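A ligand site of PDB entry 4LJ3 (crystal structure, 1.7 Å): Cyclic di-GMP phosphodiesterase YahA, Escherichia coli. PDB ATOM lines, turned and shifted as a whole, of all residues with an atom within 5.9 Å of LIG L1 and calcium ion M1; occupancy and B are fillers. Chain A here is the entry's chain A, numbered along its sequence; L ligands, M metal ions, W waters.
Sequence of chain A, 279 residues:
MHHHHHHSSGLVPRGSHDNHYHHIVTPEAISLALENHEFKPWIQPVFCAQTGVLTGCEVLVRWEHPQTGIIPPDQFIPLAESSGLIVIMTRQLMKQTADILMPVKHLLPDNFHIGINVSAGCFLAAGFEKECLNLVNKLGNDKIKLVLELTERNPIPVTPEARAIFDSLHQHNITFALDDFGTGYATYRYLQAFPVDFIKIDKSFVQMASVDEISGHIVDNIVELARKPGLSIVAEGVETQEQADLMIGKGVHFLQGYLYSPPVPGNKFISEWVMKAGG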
ATOM      1  N   VAL A  46      29.749   6.773  -8.955  1.00  0.00           N
ATOM      2  CA  VAL A  46      28.417   6.611  -9.469  1.00  0.00           C
ATOM      3  C   VAL A  46      28.441   5.368 -10.340  1.00  0.00           C
ATOM      4  O   VAL A  46      29.446   5.097 -11.023  1.00  0.00           O
ATOM      5  CB  VAL A  46      27.983   7.836 -10.279  1.00  0.00           C
ATOM      6  CG1 VAL A  46      26.605   7.598 -10.925  1.00  0.00           C
ATOM      7  CG2 VAL A  46      27.959   9.080  -9.408  1.00  0.00           C
ATOM      8  N   PHE A  47      27.352   4.624 -10.307  1.00  0.00           N
ATOM      9  CA  PHE A  47      27.301   3.266 -10.872  1.00  0.00           C
ATOM     10  C   PHE A  47      26.102   3.121 -11.761  1.00  0.00           C
ATOM     11  O   PHE A  47      25.071   3.741 -11.506  1.00  0.00           O
ATOM     12  CB  PHE A  47      27.206   2.193  -9.763  1.00  0.00           C
ATOM     13  CG  PHE A  47      28.342   2.274  -8.800  1.00  0.00           C
ATOM     14  CD1 PHE A  47      29.504   1.602  -9.060  1.00  0.00           C
ATOM     15  CD2 PHE A  47      28.259   3.080  -7.679  1.00  0.00           C
ATOM     16  CE1 PHE A  47      30.580   1.732  -8.190  1.00  0.00           C
ATOM     17  CE2 PHE A  47      29.337   3.232  -6.807  1.00  0.00           C
ATOM     18  CZ  PHE A  47      30.472   2.514  -7.066  1.00  0.00           C
ATOM     19  N   THR A  55      30.475   4.003 -13.524  1.00  0.00           N
ATOM     20  CA  THR A  55      30.199   4.864 -14.722  1.00  0.00           C
ATOM     21  C   THR A  55      30.711   6.297 -14.582  1.00  0.00           C
ATOM     22  O   THR A  55      30.855   7.046 -15.578  1.00  0.00           O
ATOM     23  CB  THR A  55      28.699   4.930 -15.097  1.00  0.00           C
ATOM     24  OG1 THR A  55      27.921   5.419 -14.014  1.00  0.00           O
ATOM     25  CG2 THR A  55      28.221   3.563 -15.501  1.00  0.00           C
ATOM     26  N   GLY A  56      30.988   6.684 -13.345  1.00  0.00           N
ATOM     27  CA  GLY A  56      31.293   8.071 -13.090  1.00  0.00           C
ATOM     28  C   GLY A  56      31.542   8.389 -11.649  1.00  0.00           C
ATOM     29  O   GLY A  56      31.893   7.504 -10.859  1.00  0.00           O
ATOM     30  N   CYS A  57      31.406   9.676 -11.337  1.00  0.00           N
ATOM     31  CA  CYS A  57      31.660  10.199  -9.996  1.00  0.00           C
ATOM     32  C   CYS A  57      31.076  11.597  -9.825  1.00  0.00           C
ATOM     33  O   CYS A  57      30.721  12.269 -10.808  1.00  0.00           O
ATOM     34  CB  CYS A  57      33.167  10.243  -9.737  1.00  0.00           C
ATOM     35  SG  CYS A  57      34.076  11.511 -10.664  1.00  0.00           S
ATOM     36  N   GLU A  58      30.947  12.027  -8.582  1.00  0.00           N
ATOM     37  CA  GLU A  58      30.647  13.408  -8.242  1.00  0.00           C
ATOM     38  C   GLU A  58      31.773  13.933  -7.359  1.00  0.00           C
ATOM     39  O   GLU A  58      32.212  13.271  -6.411  1.00  0.00           O
ATOM     40  CB  GLU A  58      29.312  13.547  -7.502  1.00  0.00           C
ATOM     41  CG  GLU A  58      28.975  15.026  -7.277  1.00  0.00           C
ATOM     42  CD  GLU A  58      27.705  15.252  -6.464  1.00  0.00           C
ATOM     43  OE1 GLU A  58      27.363  16.408  -6.194  1.00  0.00           O
ATOM     44  OE2 GLU A  58      27.069  14.270  -6.083  1.00  0.00           O
ATOM     45  N   LEU A  60      32.948  16.443  -4.546  1.00  0.00           N
ATOM     46  CA  LEU A  60      32.343  17.130  -3.420  1.00  0.00           C
ATOM     47  C   LEU A  60      33.460  17.757  -2.640  1.00  0.00           C
ATOM     48  O   LEU A  60      34.425  17.054  -2.315  1.00  0.00           O
ATOM     49  CB  LEU A  60      31.575  16.161  -2.550  1.00  0.00           C
ATOM     50  CG  LEU A  60      30.307  15.722  -3.304  1.00  0.00           C
ATOM     51  CD1 LEU A  60      29.768  14.392  -2.805  1.00  0.00           C
ATOM     52  CD2 LEU A  60      29.260  16.788  -3.214  1.00  0.00           C
ATOM     53  N   HIS A 113      31.819   9.682 -16.414  1.00  0.00           N
ATOM     54  CA  HIS A 113      31.208  10.991 -16.123  1.00  0.00           C
ATOM     55  C   HIS A 113      31.849  11.624 -14.901  1.00  0.00           C
ATOM     56  O   HIS A 113      31.994  10.961 -13.881  1.00  0.00           O
ATOM     57  CB  HIS A 113      29.726  10.879 -15.783  1.00  0.00           C
ATOM     58  CG  HIS A 113      28.885  10.203 -16.813  1.00  0.00           C
ATOM     59  ND1 HIS A 113      28.909   8.847 -17.025  1.00  0.00           N
ATOM     60  CD2 HIS A 113      27.934  10.701 -17.635  1.00  0.00           C
ATOM     61  CE1 HIS A 113      28.025   8.526 -17.956  1.00  0.00           C
ATOM     62  NE2 HIS A 113      27.430   9.632 -18.350  1.00  0.00           N
ATOM     63  N   ILE A 114      32.170  12.910 -15.000  1.00  0.00           N
ATOM     64  CA  ILE A 114      32.679  13.666 -13.842  1.00  0.00           C
ATOM     65  C   ILE A 114      31.718  14.747 -13.507  1.00  0.00           C
ATOM     66  O   ILE A 114      31.599  15.745 -14.244  1.00  0.00           O
ATOM     67  CB  ILE A 114      34.069  14.271 -14.107  1.00  0.00           C
ATOM     68  CG1 ILE A 114      35.084  13.147 -14.362  1.00  0.00           C
ATOM     69  CG2 ILE A 114      34.506  15.152 -12.930  1.00  0.00           C
ATOM     70  CD1 ILE A 114      36.356  13.638 -15.024  1.00  0.00           C
ATOM     71  N   GLY A 115      31.028  14.587 -12.382  1.00  0.00           N
ATOM     72  CA  GLY A 115      30.082  15.579 -11.885  1.00  0.00           C
ATOM     73  C   GLY A 115      30.704  16.690 -11.054  1.00  0.00           C
ATOM     74  O   GLY A 115      31.365  16.400 -10.043  1.00  0.00           O
ATOM     75  N   ASN A 117      29.718  20.280  -9.075  1.00  0.00           N
ATOM     76  CA  ASN A 117      28.679  21.191  -8.623  1.00  0.00           C
ATOM     77  C   ASN A 117      28.973  22.595  -9.039  1.00  0.00           C
ATOM     78  O   ASN A 117      29.944  23.164  -8.575  1.00  0.00           O
ATOM     79  CB  ASN A 117      28.509  21.100  -7.122  1.00  0.00           C
ATOM     80  CG  ASN A 117      27.967  19.759  -6.727  1.00  0.00           C
ATOM     81  OD1 ASN A 117      26.782  19.461  -6.948  1.00  0.00           O
ATOM     82  ND2 ASN A 117      28.824  18.921  -6.204  1.00  0.00           N
ATOM     83  N   VAL A 147      30.045  16.633 -16.480  1.00  0.00           N
ATOM     84  CA  VAL A 147      28.646  16.875 -16.116  1.00  0.00           C
ATOM     85  C   VAL A 147      28.593  18.015 -15.121  1.00  0.00           C
ATOM     86  O   VAL A 147      29.150  17.952 -14.009  1.00  0.00           O
ATOM     87  CB  VAL A 147      27.959  15.628 -15.505  1.00  0.00           C
ATOM     88  CG1 VAL A 147      26.498  15.945 -15.218  1.00  0.00           C
ATOM     89  CG2 VAL A 147      28.115  14.421 -16.416  1.00  0.00           C
ATOM     90  N   GLU A 149      26.607  19.964 -12.579  1.00  0.00           N
ATOM     91  CA  GLU A 149      25.451  19.754 -11.716  1.00  0.00           C
ATOM     92  C   GLU A 149      24.927  21.099 -11.238  1.00  0.00           C
ATOM     93  O   GLU A 149      25.625  21.811 -10.530  1.00  0.00           O
ATOM     94  CB  GLU A 149      25.804  18.837 -10.557  1.00  0.00           C
ATOM     95  CG  GLU A 149      26.345  17.484 -11.021  1.00  0.00           C
ATOM     96  CD  GLU A 149      26.260  16.372  -9.965  1.00  0.00           C
ATOM     97  OE1 GLU A 149      25.722  16.634  -8.872  1.00  0.00           O
ATOM     98  OE2 GLU A 149      26.656  15.210 -10.242  1.00  0.00           O
ATOM     99  N   ALA A 177      23.508  18.230 -15.213  1.00  0.00           N
ATOM    100  CA  ALA A 177      22.541  17.529 -14.362  1.00  0.00           C
ATOM    101  C   ALA A 177      21.742  18.529 -13.542  1.00  0.00           C
ATOM    102  O   ALA A 177      22.266  19.575 -13.156  1.00  0.00           O
ATOM    103  CB  ALA A 177      23.213  16.547 -13.423  1.00  0.00           C
ATOM    104  N   ASP A 179      20.425  18.825  -9.860  1.00  0.00           N
ATOM    105  CA  ASP A 179      20.447  18.340  -8.485  1.00  0.00           C
ATOM    106  C   ASP A 179      19.085  18.439  -7.777  1.00  0.00           C
ATOM    107  O   ASP A 179      18.263  19.293  -8.121  1.00  0.00           O
ATOM    108  CB  ASP A 179      21.413  19.216  -7.646  1.00  0.00           C
ATOM    109  CG  ASP A 179      22.803  18.622  -7.499  1.00  0.00           C
ATOM    110  OD1 ASP A 179      22.962  17.388  -7.326  1.00  0.00           O
ATOM    111  OD2 ASP A 179      23.742  19.414  -7.501  1.00  0.00           O
ATOM    112  N   PHE A 198      20.727  15.012 -17.296  1.00  0.00           N
ATOM    113  CA  PHE A 198      20.521  14.067 -16.216  1.00  0.00           C
ATOM    114  C   PHE A 198      19.676  14.723 -15.148  1.00  0.00           C
ATOM    115  O   PHE A 198      19.820  15.926 -14.900  1.00  0.00           O
ATOM    116  CB  PHE A 198      21.863  13.699 -15.550  1.00  0.00           C
ATOM    117  CG  PHE A 198      22.867  13.120 -16.480  1.00  0.00           C
ATOM    118  CD1 PHE A 198      23.761  13.930 -17.139  1.00  0.00           C
ATOM    119  CD2 PHE A 198      22.954  11.766 -16.654  1.00  0.00           C
ATOM    120  CE1 PHE A 198      24.691  13.396 -18.011  1.00  0.00           C
ATOM    121  CE2 PHE A 198      23.875  11.225 -17.533  1.00  0.00           C
ATOM    122  CZ  PHE A 198      24.768  12.044 -18.188  1.00  0.00           C
ATOM    123  N   LYS A 200      18.880  14.194 -11.086  1.00  0.00           N
ATOM    124  CA  LYS A 200      19.290  13.527  -9.861  1.00  0.00           C
ATOM    125  C   LYS A 200      18.163  13.692  -8.848  1.00  0.00           C
ATOM    126  O   LYS A 200      17.869  14.803  -8.369  1.00  0.00           O
ATOM    127  CB  LYS A 200      20.574  14.123  -9.266  1.00  0.00           C
ATOM    128  CG  LYS A 200      21.686  14.338 -10.264  1.00  0.00           C
ATOM    129  CD  LYS A 200      23.035  14.566  -9.598  1.00  0.00           C
ATOM    130  CE  LYS A 200      23.699  13.304  -9.084  1.00  0.00           C
ATOM    131  NZ  LYS A 200      25.028  13.617  -8.451  1.00  0.00           N
ATOM    132  N   VAL A 234      19.482   9.706 -12.036  1.00  0.00           N
ATOM    133  CA  VAL A 234      20.404   9.240 -11.027  1.00  0.00           C
ATOM    134  C   VAL A 234      19.652   9.252  -9.719  1.00  0.00           C
ATOM    135  O   VAL A 234      19.070  10.263  -9.343  1.00  0.00           O
ATOM    136  CB  VAL A 234      21.643  10.172 -10.875  1.00  0.00           C
ATOM    137  CG1 VAL A 234      22.683   9.522  -9.961  1.00  0.00           C
ATOM    138  CG2 VAL A 234      22.324  10.445 -12.205  1.00  0.00           C
ATOM    139  N   GLU A 236      20.416   9.445  -6.083  1.00  0.00           N
ATOM    140  CA  GLU A 236      21.483   9.782  -5.195  1.00  0.00           C
ATOM    141  C   GLU A 236      20.981   9.563  -3.769  1.00  0.00           C
ATOM    142  O   GLU A 236      19.758   9.598  -3.456  1.00  0.00           O
ATOM    143  CB  GLU A 236      21.943  11.199  -5.421  1.00  0.00           C
ATOM    144  CG  GLU A 236      20.780  12.125  -5.538  1.00  0.00           C
ATOM    145  CD  GLU A 236      21.024  13.415  -4.842  1.00  0.00           C
ATOM    146  OE1 GLU A 236      22.169  13.971  -5.008  1.00  0.00           O
ATOM    147  OE2 GLU A 236      20.094  13.842  -4.128  1.00  0.00           O
ATOM    148  N   PHE A 254      21.280   5.358 -13.018  1.00  0.00           N
ATOM    149  CA  PHE A 254      22.506   5.429 -12.221  1.00  0.00           C
ATOM    150  C   PHE A 254      22.170   5.463 -10.747  1.00  0.00           C
ATOM    151  O   PHE A 254      21.148   5.957 -10.366  1.00  0.00           O
ATOM    152  CB  PHE A 254      23.264   6.684 -12.572  1.00  0.00           C
ATOM    153  CG  PHE A 254      23.695   6.744 -14.006  1.00  0.00           C
ATOM    154  CD1 PHE A 254      24.750   5.948 -14.460  1.00  0.00           C
ATOM    155  CD2 PHE A 254      23.074   7.578 -14.902  1.00  0.00           C
ATOM    156  CE1 PHE A 254      25.140   5.990 -15.799  1.00  0.00           C
ATOM    157  CE2 PHE A 254      23.481   7.661 -16.211  1.00  0.00           C
ATOM    158  CZ  PHE A 254      24.493   6.834 -16.674  1.00  0.00           C
ATOM    159  N   GLN A 256      24.025   6.271  -6.745  1.00  0.00           N
ATOM    160  CA  GLN A 256      25.084   6.980  -6.013  1.00  0.00           C
ATOM    161  C   GLN A 256      24.684   6.972  -4.550  1.00  0.00           C
ATOM    162  O   GLN A 256      23.539   7.282  -4.234  1.00  0.00           O
ATOM    163  CB  GLN A 256      25.181   8.422  -6.529  1.00  0.00           C
ATOM    164  CG  GLN A 256      26.285   9.259  -5.925  1.00  0.00           C
ATOM    165  CD  GLN A 256      26.277  10.687  -6.379  1.00  0.00           C
ATOM    166  OE1 GLN A 256      25.665  11.026  -7.392  1.00  0.00           O
ATOM    167  NE2 GLN A 256      26.982  11.534  -5.665  1.00  0.00           N
HETATM  168  C1  LIG L   1      25.974  12.725 -12.436  1.00  0.00           C
HETATM  169  C2  LIG L   1      25.467  12.319 -13.794  1.00  0.00           C
HETATM  170  C3  LIG L   1      25.516  10.840 -13.824  1.00  0.00           C
HETATM  171  C4  LIG L   1      26.899  10.391 -13.876  1.00  0.00           C
HETATM  172  C5  LIG L   1      27.627  10.856 -12.596  1.00  0.00           C
HETATM  173  C6  LIG L   1      27.416  12.373 -12.352  1.00  0.00           C
HETATM  174  C7  LIG L   1      26.858   8.874 -14.153  1.00  0.00           C
HETATM  175  O1  LIG L   1      28.068   8.245 -13.805  1.00  0.00           O
HETATM  176  O2  LIG L   1      25.827  14.116 -12.396  1.00  0.00           O
HETATM  177  P1  LG2 L   2      24.545  17.513  -3.364  1.00  0.00           P
HETATM  178  O1  LG2 L   2      24.900  18.196  -4.644  1.00  0.00           O
HETATM  179  O2  LG2 L   2      23.123  17.038  -3.254  1.00  0.00           O
HETATM  180  O3  LG2 L   2      25.566  16.326  -3.133  1.00  0.00           O
HETATM  181  C1  LG2 L   2      25.239  15.102  -2.484  1.00  0.00           C
HETATM  182  C2  LG2 L   2      25.380  15.204  -0.987  1.00  0.00           C
HETATM  183  O4  LG2 L   2      24.745  14.058  -0.433  1.00  0.00           O
HETATM  184  C3  LG2 L   2      26.825  15.175  -0.515  1.00  0.00           C
HETATM  185  O5  LG2 L   2      26.979  15.804   0.752  1.00  0.00           O
HETATM  186  C4  LG2 L   2      27.076  13.678  -0.420  1.00  0.00           C
HETATM  187  O6  LG2 L   2      28.224  13.273   0.346  1.00  0.00           O
HETATM  188  C5  LG2 L   2      25.760  13.297   0.227  1.00  0.00           C
HETATM  189  N1  LG2 L   2      25.412  11.885   0.076  1.00  0.00           N
HETATM  190  C6  LG2 L   2      25.679  11.077  -0.991  1.00  0.00           C
HETATM  191  N2  LG2 L   2      25.227   9.840  -0.781  1.00  0.00           N
HETATM  192  C7  LG2 L   2      24.605   9.888   0.426  1.00  0.00           C
HETATM  193  C8  LG2 L   2      23.898   8.894   1.220  1.00  0.00           C
HETATM  194  O7  LG2 L   2      23.795   7.737   0.784  1.00  0.00           O
HETATM  195  N3  LG2 L   2      23.455   9.278   2.405  1.00  0.00           N
HETATM  196  C9  LG2 L   2      23.593  10.541   2.877  1.00  0.00           C
HETATM  197  N4  LG2 L   2      23.073  10.822   4.060  1.00  0.00           N
HETATM  198  N5  LG2 L   2      24.229  11.549   2.221  1.00  0.00           N
HETATM  199  C10 LG2 L   2      24.738  11.227   0.987  1.00  0.00           C
HETATM  200  P2  LG2 L   2      28.161  16.857   1.012  1.00  0.00           P
HETATM  201  O8  LG2 L   2      28.023  17.234   2.475  1.00  0.00           O
HETATM  202  O9  LG2 L   2      29.412  16.518   0.321  1.00  0.00           O
HETATM  203  O10 LG2 L   2      27.562  18.074   0.147  1.00  0.00           O
HETATM  204  C11 LG2 L   2      26.427  18.786   0.584  1.00  0.00           C
HETATM  205  C12 LG2 L   2      26.019  19.746  -0.511  1.00  0.00           C
HETATM  206  O11 LG2 L   2      27.071  20.721  -0.633  1.00  0.00           O
HETATM  207  C13 LG2 L   2      25.850  19.190  -1.911  1.00  0.00           C
HETATM  208  O12 LG2 L   2      24.602  18.497  -2.101  1.00  0.00           O
HETATM  209  C14 LG2 L   2      26.072  20.473  -2.711  1.00  0.00           C
HETATM  210  O13 LG2 L   2      24.853  21.209  -2.798  1.00  0.00           O
HETATM  211  C15 LG2 L   2      27.097  21.286  -1.922  1.00  0.00           C
HETATM  212  N6  LG2 L   2      28.425  21.120  -2.510  1.00  0.00           N
HETATM  213  C16 LG2 L   2      29.278  20.086  -2.316  1.00  0.00           C
HETATM  214  N7  LG2 L   2      30.403  20.261  -3.055  1.00  0.00           N
HETATM  215  C17 LG2 L   2      30.232  21.406  -3.728  1.00  0.00           C
HETATM  216  C18 LG2 L   2      30.994  22.219  -4.688  1.00  0.00           C
HETATM  217  O14 LG2 L   2      32.127  21.852  -5.065  1.00  0.00           O
HETATM  218  N8  LG2 L   2      30.462  23.375  -5.128  1.00  0.00           N
HETATM  219  C19 LG2 L   2      29.251  23.812  -4.777  1.00  0.00           C
HETATM  220  N9  LG2 L   2      28.829  24.982  -5.301  1.00  0.00           N
HETATM  221  N10 LG2 L   2      28.470  23.137  -3.904  1.00  0.00           N
HETATM  222  C20 LG2 L   2      28.930  21.971  -3.364  1.00  0.00           C
HETATM  223 CA    CA M   1      25.279  17.489  -6.759  1.00  0.00          CA
HETATM  224 CA    CA M   2      21.212  15.786  -3.415  1.00  0.00          CA
HETATM  225  O   HOH W   1      24.684  15.310  -6.071  1.00  0.00           O
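The nearest printed residue that does not touch calcium ion M1 is Lys 200 (4.2 Å).
The backbone carbonyl oxygen of Val 46 sits at hydrogen-bond distance from the backbone NH of Thr 55 (2.9 Å). NZ of Lys 200 lies within hydrogen-bond range of OE1 of Gln 256 (2.9 Å). The side-chain amide nitrogen (NE2) of Gln 256 lies within hydrogen-bond range of the side-chain carboxylate (OE2) of Glu 58 (2.8 Å). The backbone NH of His 113 lies within hydrogen-bond range of the backbone carbonyl oxygen of Thr 55. The side-chain carboxylate (OE2) of Glu 58 is in salt-bridge range of the side-chain amino group (NZ) of Lys 200 (3.2 Å). O of His 113 sits at hydrogen-bond distance from N of Cys 57 (2.9 Å). The side-chain carboxylate (OE2) of Glu 149 lies within salt-bridge range of the side-chain amino group (NZ) of Lys 200 (2.9 Å). N of Gly 115 sits at hydrogen-bond distance from O of Cys 57 (2.8 Å).
Calcium ion M1 is bound by an oxygen (O1) of LG2 L2 (2.3 Å), the side-chain carboxylate (OE1) of Glu 149 (2.3 Å), water W1 (2.4 Å), the side-chain carboxylate (OD1) of Asp 179 (2.4 Å), the side-chain carboxylate (OE1) of Glu 58 (2.4 Å), the side-chain amide oxygen (OD1) of Asn 117 (2.5 Å) and the side-chain carboxylate (OD2) of Asp 179 (2.6 Å).
Water W1 lies within hydrogen-bond range of OE2 of Glu 58 (2.6 Å), NZ of Lys 200 (2.9 Å) and O3 of LG2 L2 (3.2 Å).
O1 of LIG L1 sits at hydrogen-bond distance from ND1 of His 113, 3.4 Å away. N of Gly 56 lies close to O1 of LIG L1 (3.3 Å). O of Asn 117 lies within hydrogen-bond range of N8 of LG2 L2 (3.5 Å). The side-chain hydroxyl of Thr 55 sits at hydrogen-bond distance from an oxygen (O1) of LIG L1 (2.8 Å). The side-chain carboxylate (OE2) of Glu 149 sits at hydrogen-bond distance from an oxygen (O2) of LIG L1 (2.6 Å).
CG1 of Val 46 touches O1 of LIG L1, 3.3 Å away. Cys 57 touches LIG L1 (O to C6, 3.6 Å). Val 147 touches LIG L1 (CG1 to O2, 3.4 Å). Ala 177 touches LIG L1. Phe 198 touches LIG L1. CD of Lys 200 touches O2 of LIG L1, at 3.98 Å. Val 234 touches LIG L1. Phe 254 touches LIG L1 (CD1 to C7, 3.6 Å). Hydrophobic or aromatic side chains that line LIG L1: Val 46, His 113, Val 147, Ala 177, Phe 198, Val 234 and Phe 254. 12 residues have an atom within 4 Å of LIG L1: Val 46, Thr 55, Gly 56, Cys 57, His 113, Val 147, Glu 149, Ala 177, Phe 198, Lys 200, Val 234 and Phe 254.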
